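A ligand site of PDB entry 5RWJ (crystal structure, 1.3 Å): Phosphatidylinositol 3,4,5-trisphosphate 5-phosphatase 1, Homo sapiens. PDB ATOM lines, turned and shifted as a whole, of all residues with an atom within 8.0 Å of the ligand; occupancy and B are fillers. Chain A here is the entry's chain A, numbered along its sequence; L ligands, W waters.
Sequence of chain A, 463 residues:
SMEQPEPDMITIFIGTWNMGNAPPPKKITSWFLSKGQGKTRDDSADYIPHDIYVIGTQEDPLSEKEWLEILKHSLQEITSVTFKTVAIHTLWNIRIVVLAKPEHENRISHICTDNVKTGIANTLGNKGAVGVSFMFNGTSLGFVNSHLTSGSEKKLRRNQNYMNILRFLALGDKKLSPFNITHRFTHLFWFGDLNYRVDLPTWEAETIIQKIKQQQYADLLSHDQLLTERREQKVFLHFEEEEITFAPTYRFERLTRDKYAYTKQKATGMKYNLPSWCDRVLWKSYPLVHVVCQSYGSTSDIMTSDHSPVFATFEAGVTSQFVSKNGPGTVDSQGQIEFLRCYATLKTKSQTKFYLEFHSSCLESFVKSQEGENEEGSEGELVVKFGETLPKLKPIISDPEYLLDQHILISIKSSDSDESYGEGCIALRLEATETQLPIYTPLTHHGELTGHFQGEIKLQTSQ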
ATOM      1  N   LYS A  72      32.677 -24.583  34.010  1.00  0.00           N
ATOM      2  CA  LYS A  72      33.801 -24.513  33.060  1.00  0.00           C
ATOM      3  C   LYS A  72      35.155 -24.440  33.777  1.00  0.00           C
ATOM      4  O   LYS A  72      36.136 -25.116  33.367  1.00  0.00           O
ATOM      5  CB  LYS A  72      33.617 -23.344  32.111  1.00  0.00           C
ATOM      6  CG  LYS A  72      32.590 -23.591  31.073  1.00  0.00           C
ATOM      7  CD  LYS A  72      32.861 -22.728  29.909  1.00  0.00           C
ATOM      8  CE  LYS A  72      31.802 -23.055  28.926  1.00  0.00           C
ATOM      9  NZ  LYS A  72      32.122 -22.571  27.590  1.00  0.00           N
ATOM     10  N   PHE A  83      36.094 -26.215  27.878  1.00  0.00           N
ATOM     11  CA  PHE A  83      34.946 -26.871  27.199  1.00  0.00           C
ATOM     12  C   PHE A  83      34.091 -25.810  26.501  1.00  0.00           C
ATOM     13  O   PHE A  83      33.987 -24.709  27.019  1.00  0.00           O
ATOM     14  CB  PHE A  83      34.160 -27.696  28.233  1.00  0.00           C
ATOM     15  CG  PHE A  83      34.760 -29.056  28.466  1.00  0.00           C
ATOM     16  CD1 PHE A  83      35.902 -29.209  29.214  1.00  0.00           C
ATOM     17  CD2 PHE A  83      34.187 -30.147  27.859  1.00  0.00           C
ATOM     18  CE1 PHE A  83      36.497 -30.468  29.314  1.00  0.00           C
ATOM     19  CE2 PHE A  83      34.763 -31.400  27.984  1.00  0.00           C
ATOM     20  CZ  PHE A  83      35.930 -31.538  28.687  1.00  0.00           C
ATOM     21  N   LYS A  84      33.433 -26.196  25.448  1.00  0.00           N
ATOM     22  CA  LYS A  84      32.455 -25.358  24.747  1.00  0.00           C
ATOM     23  C   LYS A  84      31.063 -25.652  25.270  1.00  0.00           C
ATOM     24  O   LYS A  84      30.730 -26.814  25.576  1.00  0.00           O
ATOM     25  CB  LYS A  84      32.450 -25.643  23.265  1.00  0.00           C
ATOM     26  CG  LYS A  84      33.786 -25.370  22.605  1.00  0.00           C
ATOM     27  CD  LYS A  84      34.102 -23.925  22.478  1.00  0.00           C
ATOM     28  CE  LYS A  84      35.291 -23.684  21.584  1.00  0.00           C
ATOM     29  NZ  LYS A  84      35.753 -22.293  21.726  1.00  0.00           N
ATOM     30  N   THR A  85      30.234 -24.627  25.368  1.00  0.00           N
ATOM     31  CA  THR A  85      28.847 -24.769  25.797  1.00  0.00           C
ATOM     32  C   THR A  85      28.000 -25.150  24.606  1.00  0.00           C
ATOM     33  O   THR A  85      27.794 -24.342  23.677  1.00  0.00           O
ATOM     34  CB  THR A  85      28.341 -23.470  26.441  1.00  0.00           C
ATOM     35  OG1 THR A  85      29.294 -23.042  27.406  1.00  0.00           O
ATOM     36  CG2 THR A  85      26.956 -23.618  27.033  1.00  0.00           C
ATOM     37  N   VAL A  86      27.424 -26.345  24.635  1.00  0.00           N
ATOM     38  CA  VAL A  86      26.499 -26.838  23.596  1.00  0.00           C
ATOM     39  C   VAL A  86      25.121 -26.243  23.811  1.00  0.00           C
ATOM     40  O   VAL A  86      24.475 -25.757  22.865  1.00  0.00           O
ATOM     41  CB  VAL A  86      26.427 -28.380  23.629  1.00  0.00           C
ATOM     42  CG1 VAL A  86      25.406 -28.897  22.658  1.00  0.00           C
ATOM     43  CG2 VAL A  86      27.796 -28.994  23.420  1.00  0.00           C
ATOM     44  N   ALA A  87      24.644 -26.262  25.061  1.00  0.00           N
ATOM     45  CA  ALA A  87      23.291 -25.809  25.368  1.00  0.00           C
ATOM     46  C   ALA A  87      23.150 -25.601  26.863  1.00  0.00           C
ATOM     47  O   ALA A  87      23.856 -26.238  27.650  1.00  0.00           O
ATOM     48  CB  ALA A  87      22.268 -26.840  24.931  1.00  0.00           C
ATOM     49  N   VAL A  98      24.934 -28.615  28.855  1.00  0.00           N
ATOM     50  CA  VAL A  98      25.739 -29.581  28.084  1.00  0.00           C
ATOM     51  C   VAL A  98      27.012 -28.883  27.637  1.00  0.00           C
ATOM     52  O   VAL A  98      26.916 -27.823  26.974  1.00  0.00           O
ATOM     53  CB  VAL A  98      24.943 -30.107  26.887  1.00  0.00           C
ATOM     54  CG1 VAL A  98      25.799 -31.072  26.102  1.00  0.00           C
ATOM     55  CG2 VAL A  98      23.646 -30.763  27.349  1.00  0.00           C
ATOM     56  N   LEU A  99      28.118 -29.485  27.969  1.00  0.00           N
ATOM     57  CA  LEU A  99      29.458 -29.018  27.620  1.00  0.00           C
ATOM     58  C   LEU A  99      30.147 -30.084  26.792  1.00  0.00           C
ATOM     59  O   LEU A  99      29.960 -31.293  27.030  1.00  0.00           O
ATOM     60  CB  LEU A  99      30.256 -28.743  28.873  1.00  0.00           C
ATOM     61  CG  LEU A  99      29.615 -27.778  29.878  1.00  0.00           C
ATOM     62  CD1 LEU A  99      30.493 -27.638  31.107  1.00  0.00           C
ATOM     63  CD2 LEU A  99      29.283 -26.423  29.276  1.00  0.00           C
ATOM     64  N   ALA A 100      30.963 -29.691  25.830  1.00  0.00           N
ATOM     65  CA  ALA A 100      31.674 -30.678  24.991  1.00  0.00           C
ATOM     66  C   ALA A 100      33.092 -30.231  24.751  1.00  0.00           C
ATOM     67  O   ALA A 100      33.404 -29.040  24.752  1.00  0.00           O
ATOM     68  CB  ALA A 100      30.974 -30.884  23.695  1.00  0.00           C
ATOM     69  N   LYS A 101      33.982 -31.195  24.535  1.00  0.00           N
ATOM     70  CA  LYS A 101      35.379 -30.867  24.180  1.00  0.00           C
ATOM     71  C   LYS A 101      35.377 -30.039  22.901  1.00  0.00           C
ATOM     72  O   LYS A 101      34.551 -30.274  22.007  1.00  0.00           O
ATOM     73  CB  LYS A 101      36.192 -32.135  23.940  1.00  0.00           C
ATOM     74  CG  LYS A 101      36.314 -33.025  25.160  1.00  0.00           C
ATOM     75  CD  LYS A 101      37.211 -34.208  24.922  1.00  0.00           C
ATOM     76  CE  LYS A 101      38.635 -33.816  24.605  1.00  0.00           C
ATOM     77  NZ  LYS A 101      39.452 -35.004  24.321  1.00  0.00           N
ATOM     78  N   PRO A 102      36.294 -29.047  22.768  1.00  0.00           N
ATOM     79  CA  PRO A 102      36.331 -28.212  21.578  1.00  0.00           C
ATOM     80  C   PRO A 102      36.428 -28.971  20.260  1.00  0.00           C
ATOM     81  O   PRO A 102      35.866 -28.517  19.321  1.00  0.00           O
ATOM     82  CB  PRO A 102      37.613 -27.424  21.761  1.00  0.00           C
ATOM     83  CG  PRO A 102      37.976 -27.492  23.195  1.00  0.00           C
ATOM     84  CD  PRO A 102      37.310 -28.716  23.780  1.00  0.00           C
ATOM     85  N   HIS A 104      34.903 -31.415  19.356  1.00  0.00           N
ATOM     86  CA  HIS A 104      33.588 -31.942  18.986  1.00  0.00           C
ATOM     87  C   HIS A 104      32.658 -30.893  18.433  1.00  0.00           C
ATOM     88  O   HIS A 104      31.534 -31.201  18.013  1.00  0.00           O
ATOM     89  CB  HIS A 104      32.935 -32.634  20.177  1.00  0.00           C
ATOM     90  CG  HIS A 104      33.701 -33.840  20.559  1.00  0.00           C
ATOM     91  ND1 HIS A 104      34.364 -34.617  19.618  1.00  0.00           N
ATOM     92  CD2 HIS A 104      33.872 -34.397  21.774  1.00  0.00           C
ATOM     93  CE1 HIS A 104      34.931 -35.631  20.282  1.00  0.00           C
ATOM     94  NE2 HIS A 104      34.612 -35.536  21.613  1.00  0.00           N
ATOM     95  N   GLU A 105      33.077 -29.626  18.440  1.00  0.00           N
ATOM     96  CA  GLU A 105      32.130 -28.545  18.109  1.00  0.00           C
ATOM     97  C   GLU A 105      31.507 -28.738  16.716  1.00  0.00           C
ATOM     98  O   GLU A 105      30.320 -28.559  16.537  1.00  0.00           O
ATOM     99  CB  GLU A 105      32.802 -27.176  18.246  1.00  0.00           C
ATOM    100  CG  GLU A 105      31.867 -26.038  17.839  1.00  0.00           C
ATOM    101  CD  GLU A 105      32.466 -24.639  17.890  1.00  0.00           C
ATOM    102  OE1 GLU A 105      33.566 -24.505  18.434  1.00  0.00           O
ATOM    103  OE2 GLU A 105      31.847 -23.700  17.269  1.00  0.00           O
ATOM    104  N   ASN A 106      32.305 -29.102  15.715  1.00  0.00           N
ATOM    105  CA  ASN A 106      31.769 -29.257  14.329  1.00  0.00           C
ATOM    106  C   ASN A 106      31.091 -30.622  14.149  1.00  0.00           C
ATOM    107  O   ASN A 106      30.392 -30.765  13.138  1.00  0.00           O
ATOM    108  CB  ASN A 106      32.830 -28.976  13.256  1.00  0.00           C
ATOM    109  CG  ASN A 106      33.287 -27.542  13.273  1.00  0.00           C
ATOM    110  OD1 ASN A 106      32.466 -26.609  13.254  1.00  0.00           O
ATOM    111  ND2 ASN A 106      34.581 -27.339  13.373  1.00  0.00           N
ATOM    112  N   ARG A 107      31.233 -31.550  15.104  1.00  0.00           N
ATOM    113  CA  ARG A 107      30.547 -32.867  15.067  1.00  0.00           C
ATOM    114  C   ARG A 107      29.139 -32.723  15.632  1.00  0.00           C
ATOM    115  O   ARG A 107      28.302 -33.604  15.405  1.00  0.00           O
ATOM    116  CB  ARG A 107      31.328 -33.897  15.886  1.00  0.00           C
ATOM    117  CG  ARG A 107      32.712 -34.120  15.316  1.00  0.00           C
ATOM    118  CD  ARG A 107      33.413 -35.118  16.193  1.00  0.00           C
ATOM    119  NE  ARG A 107      34.638 -35.530  15.485  1.00  0.00           N
ATOM    120  CZ  ARG A 107      35.835 -35.535  16.002  1.00  0.00           C
ATOM    121  NH1 ARG A 107      36.097 -35.178  17.239  1.00  0.00           N
ATOM    122  NH2 ARG A 107      36.841 -35.919  15.242  1.00  0.00           N
ATOM    123  N   ILE A 108      28.816 -31.637  16.331  1.00  0.00           N
ATOM    124  CA  ILE A 108      27.562 -31.485  17.098  1.00  0.00           C
ATOM    125  C   ILE A 108      26.686 -30.509  16.352  1.00  0.00           C
ATOM    126  O   ILE A 108      27.158 -29.364  16.082  1.00  0.00           O
ATOM    127  CB  ILE A 108      27.887 -31.109  18.549  1.00  0.00           C
ATOM    128  CG1 ILE A 108      28.511 -32.286  19.270  1.00  0.00           C
ATOM    129  CG2 ILE A 108      26.629 -30.571  19.245  1.00  0.00           C
ATOM    130  CD1 ILE A 108      29.052 -31.973  20.656  1.00  0.00           C
ATOM    131  N   SER A 109      25.460 -30.831  16.067  1.00  0.00           N
ATOM    132  CA  SER A 109      24.518 -29.974  15.333  1.00  0.00           C
ATOM    133  C   SER A 109      23.095 -30.300  15.750  1.00  0.00           C
ATOM    134  O   SER A 109      22.874 -31.239  16.585  1.00  0.00           O
ATOM    135  CB  SER A 109      24.732 -30.143  13.824  1.00  0.00           C
ATOM    136  OG  SER A 109      24.279 -31.400  13.414  1.00  0.00           O
ATOM    137  N   HIS A 110      22.107 -29.665  15.183  1.00  0.00           N
ATOM    138  CA  HIS A 110      20.686 -29.944  15.438  1.00  0.00           C
ATOM    139  C   HIS A 110      20.447 -29.882  16.934  1.00  0.00           C
ATOM    140  O   HIS A 110      19.757 -30.772  17.431  1.00  0.00           O
ATOM    141  CB  HIS A 110      20.240 -31.265  14.821  1.00  0.00           C
ATOM    142  CG  HIS A 110      20.374 -31.274  13.309  1.00  0.00           C
ATOM    143  ND1 HIS A 110      21.580 -31.406  12.694  1.00  0.00           N
ATOM    144  CD2 HIS A 110      19.466 -31.095  12.343  1.00  0.00           C
ATOM    145  CE1 HIS A 110      21.395 -31.377  11.375  1.00  0.00           C
ATOM    146  NE2 HIS A 110      20.118 -31.207  11.135  1.00  0.00           N
ATOM    147  N   ILE A 111      20.830 -28.816  17.581  1.00  0.00           N
ATOM    148  CA  ILE A 111      20.735 -28.676  19.049  1.00  0.00           C
ATOM    149  C   ILE A 111      19.332 -28.214  19.327  1.00  0.00           C
ATOM    150  O   ILE A 111      18.890 -27.197  18.767  1.00  0.00           O
ATOM    151  CB  ILE A 111      21.782 -27.724  19.590  1.00  0.00           C
ATOM    152  CG1 ILE A 111      23.194 -28.212  19.293  1.00  0.00           C
ATOM    153  CG2 ILE A 111      21.524 -27.506  21.088  1.00  0.00           C
ATOM    154  CD1 ILE A 111      24.261 -27.145  19.433  1.00  0.00           C
ATOM    155  N   PHE A 134      20.761 -33.392  20.489  1.00  0.00           N
ATOM    156  CA  PHE A 134      21.601 -32.961  19.369  1.00  0.00           C
ATOM    157  C   PHE A 134      22.056 -34.180  18.632  1.00  0.00           C
ATOM    158  O   PHE A 134      21.906 -35.311  19.101  1.00  0.00           O
ATOM    159  CB  PHE A 134      22.790 -32.112  19.823  1.00  0.00           C
ATOM    160  CG  PHE A 134      23.631 -32.685  20.905  1.00  0.00           C
ATOM    161  CD1 PHE A 134      23.306 -32.420  22.224  1.00  0.00           C
ATOM    162  CD2 PHE A 134      24.781 -33.418  20.652  1.00  0.00           C
ATOM    163  CE1 PHE A 134      24.091 -32.876  23.253  1.00  0.00           C
ATOM    164  CE2 PHE A 134      25.553 -33.905  21.680  1.00  0.00           C
ATOM    165  CZ  PHE A 134      25.191 -33.614  22.992  1.00  0.00           C
ATOM    166  N   MET A 135      22.640 -33.977  17.463  1.00  0.00           N
ATOM    167  CA  MET A 135      23.313 -35.008  16.669  1.00  0.00           C
ATOM    168  C   MET A 135      24.784 -34.896  16.986  1.00  0.00           C
ATOM    169  O   MET A 135      25.369 -33.782  17.005  1.00  0.00           O
ATOM    170  CB  MET A 135      23.140 -34.767  15.174  1.00  0.00           C
ATOM    171  CG  MET A 135      21.779 -34.996  14.702  1.00  0.00           C
ATOM    172  SD  MET A 135      21.132 -36.653  14.885  1.00  0.00           S
ATOM    173  CE  MET A 135      22.302 -37.590  13.893  1.00  0.00           C
ATOM    174  N   GLN A 321      29.191 -39.508   9.978  1.00  0.00           N
ATOM    175  CA  GLN A 321      28.264 -38.893   9.005  1.00  0.00           C
ATOM    176  C   GLN A 321      28.600 -39.429   7.610  1.00  0.00           C
ATOM    177  O   GLN A 321      29.283 -38.711   6.861  1.00  0.00           O
ATOM    178  CB  GLN A 321      28.497 -37.379   8.975  1.00  0.00           C
ATOM    179  CG  GLN A 321      28.143 -36.725  10.284  1.00  0.00           C
ATOM    180  CD  GLN A 321      28.247 -35.210  10.158  1.00  0.00           C
ATOM    181  OE1 GLN A 321      27.678 -34.628   9.217  1.00  0.00           O
ATOM    182  NE2 GLN A 321      28.957 -34.563  11.063  1.00  0.00           N
HETATM  183  N1  LIG L   1      28.343 -26.525  15.909  1.00  0.00           N
HETATM  184  C1  LIG L   1      28.956 -27.510  20.077  1.00  0.00           C
HETATM  185  C2  LIG L   1      28.347 -27.429  18.809  1.00  0.00           C
HETATM  186  C3  LIG L   1      27.995 -26.209  18.297  1.00  0.00           C
HETATM  187  C4  LIG L   1      27.374 -26.152  16.914  1.00  0.00           C
HETATM  188  C5  LIG L   1      27.643 -26.718  14.592  1.00  0.00           C
HETATM  189  C6  LIG L   1      27.710 -27.615  12.255  1.00  0.00           C
HETATM  190  C7  LIG L   1      28.222 -25.055  19.046  1.00  0.00           C
HETATM  191  C8  LIG L   1      28.793 -25.140  20.312  1.00  0.00           C
HETATM  192  C9  LIG L   1      29.173 -26.377  20.796  1.00  0.00           C
HETATM  193  C10 LIG L   1      28.534 -27.434  13.646  1.00  0.00           C
HETATM  194  C11 LIG L   1      27.954 -26.482  11.593  1.00  0.00           C
HETATM  195  C12 LIG L   1      29.401 -26.116  11.966  1.00  0.00           C
HETATM  196  O1  LIG L   1      29.593 -26.695  13.413  1.00  0.00           O
HETATM  197  F1  LIG L   1      29.737 -26.485  22.047  1.00  0.00           F
HETATM  198  O   HOH W   1      24.248 -26.341  15.069  1.00  0.00           O
HETATM  199  O   HOH W   2      29.752 -24.262  15.716  1.00  0.00           O
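O1 of the ligand sits close to OD1 of Asn 106 (2.9 Å). N1 of the ligand sits at hydrogen-bond distance from O of Glu 105 (2.9 Å). A nitrogen (N1) of the ligand lies close to the backbone carbonyl oxygen (O) of Ile 108, at 3.1 Å.
O of Lys 84 sits at hydrogen-bond distance from N of Ala 100 (2.9 Å). NZ of Lys 72 sits at hydrogen-bond distance from OG1 of Thr 85, 2.9 Å away. N of Val 86 sits at hydrogen-bond distance from O of Val 98, at 2.8 Å.
O of Thr 85 sits close to F1 of the ligand. The backbone NH (N) of Val 86 sits close to a fluorine (F1) of the ligand, 3.5 Å away. Residues that only touch the ligand: Lys 84. Hydrophobic or aromatic side chains within 4 Å of the ligand: Val 86 and Ile 108. Within 4 Å of the ligand: Lys 84, Thr 85, Val 86, Glu 105, Asn 106 and Ile 108. Along chain A the residues within 4 Å of the ligand span positions 84 to 108.
Water W2 bridges OE2 of Glu 105 and N1 of the ligand.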
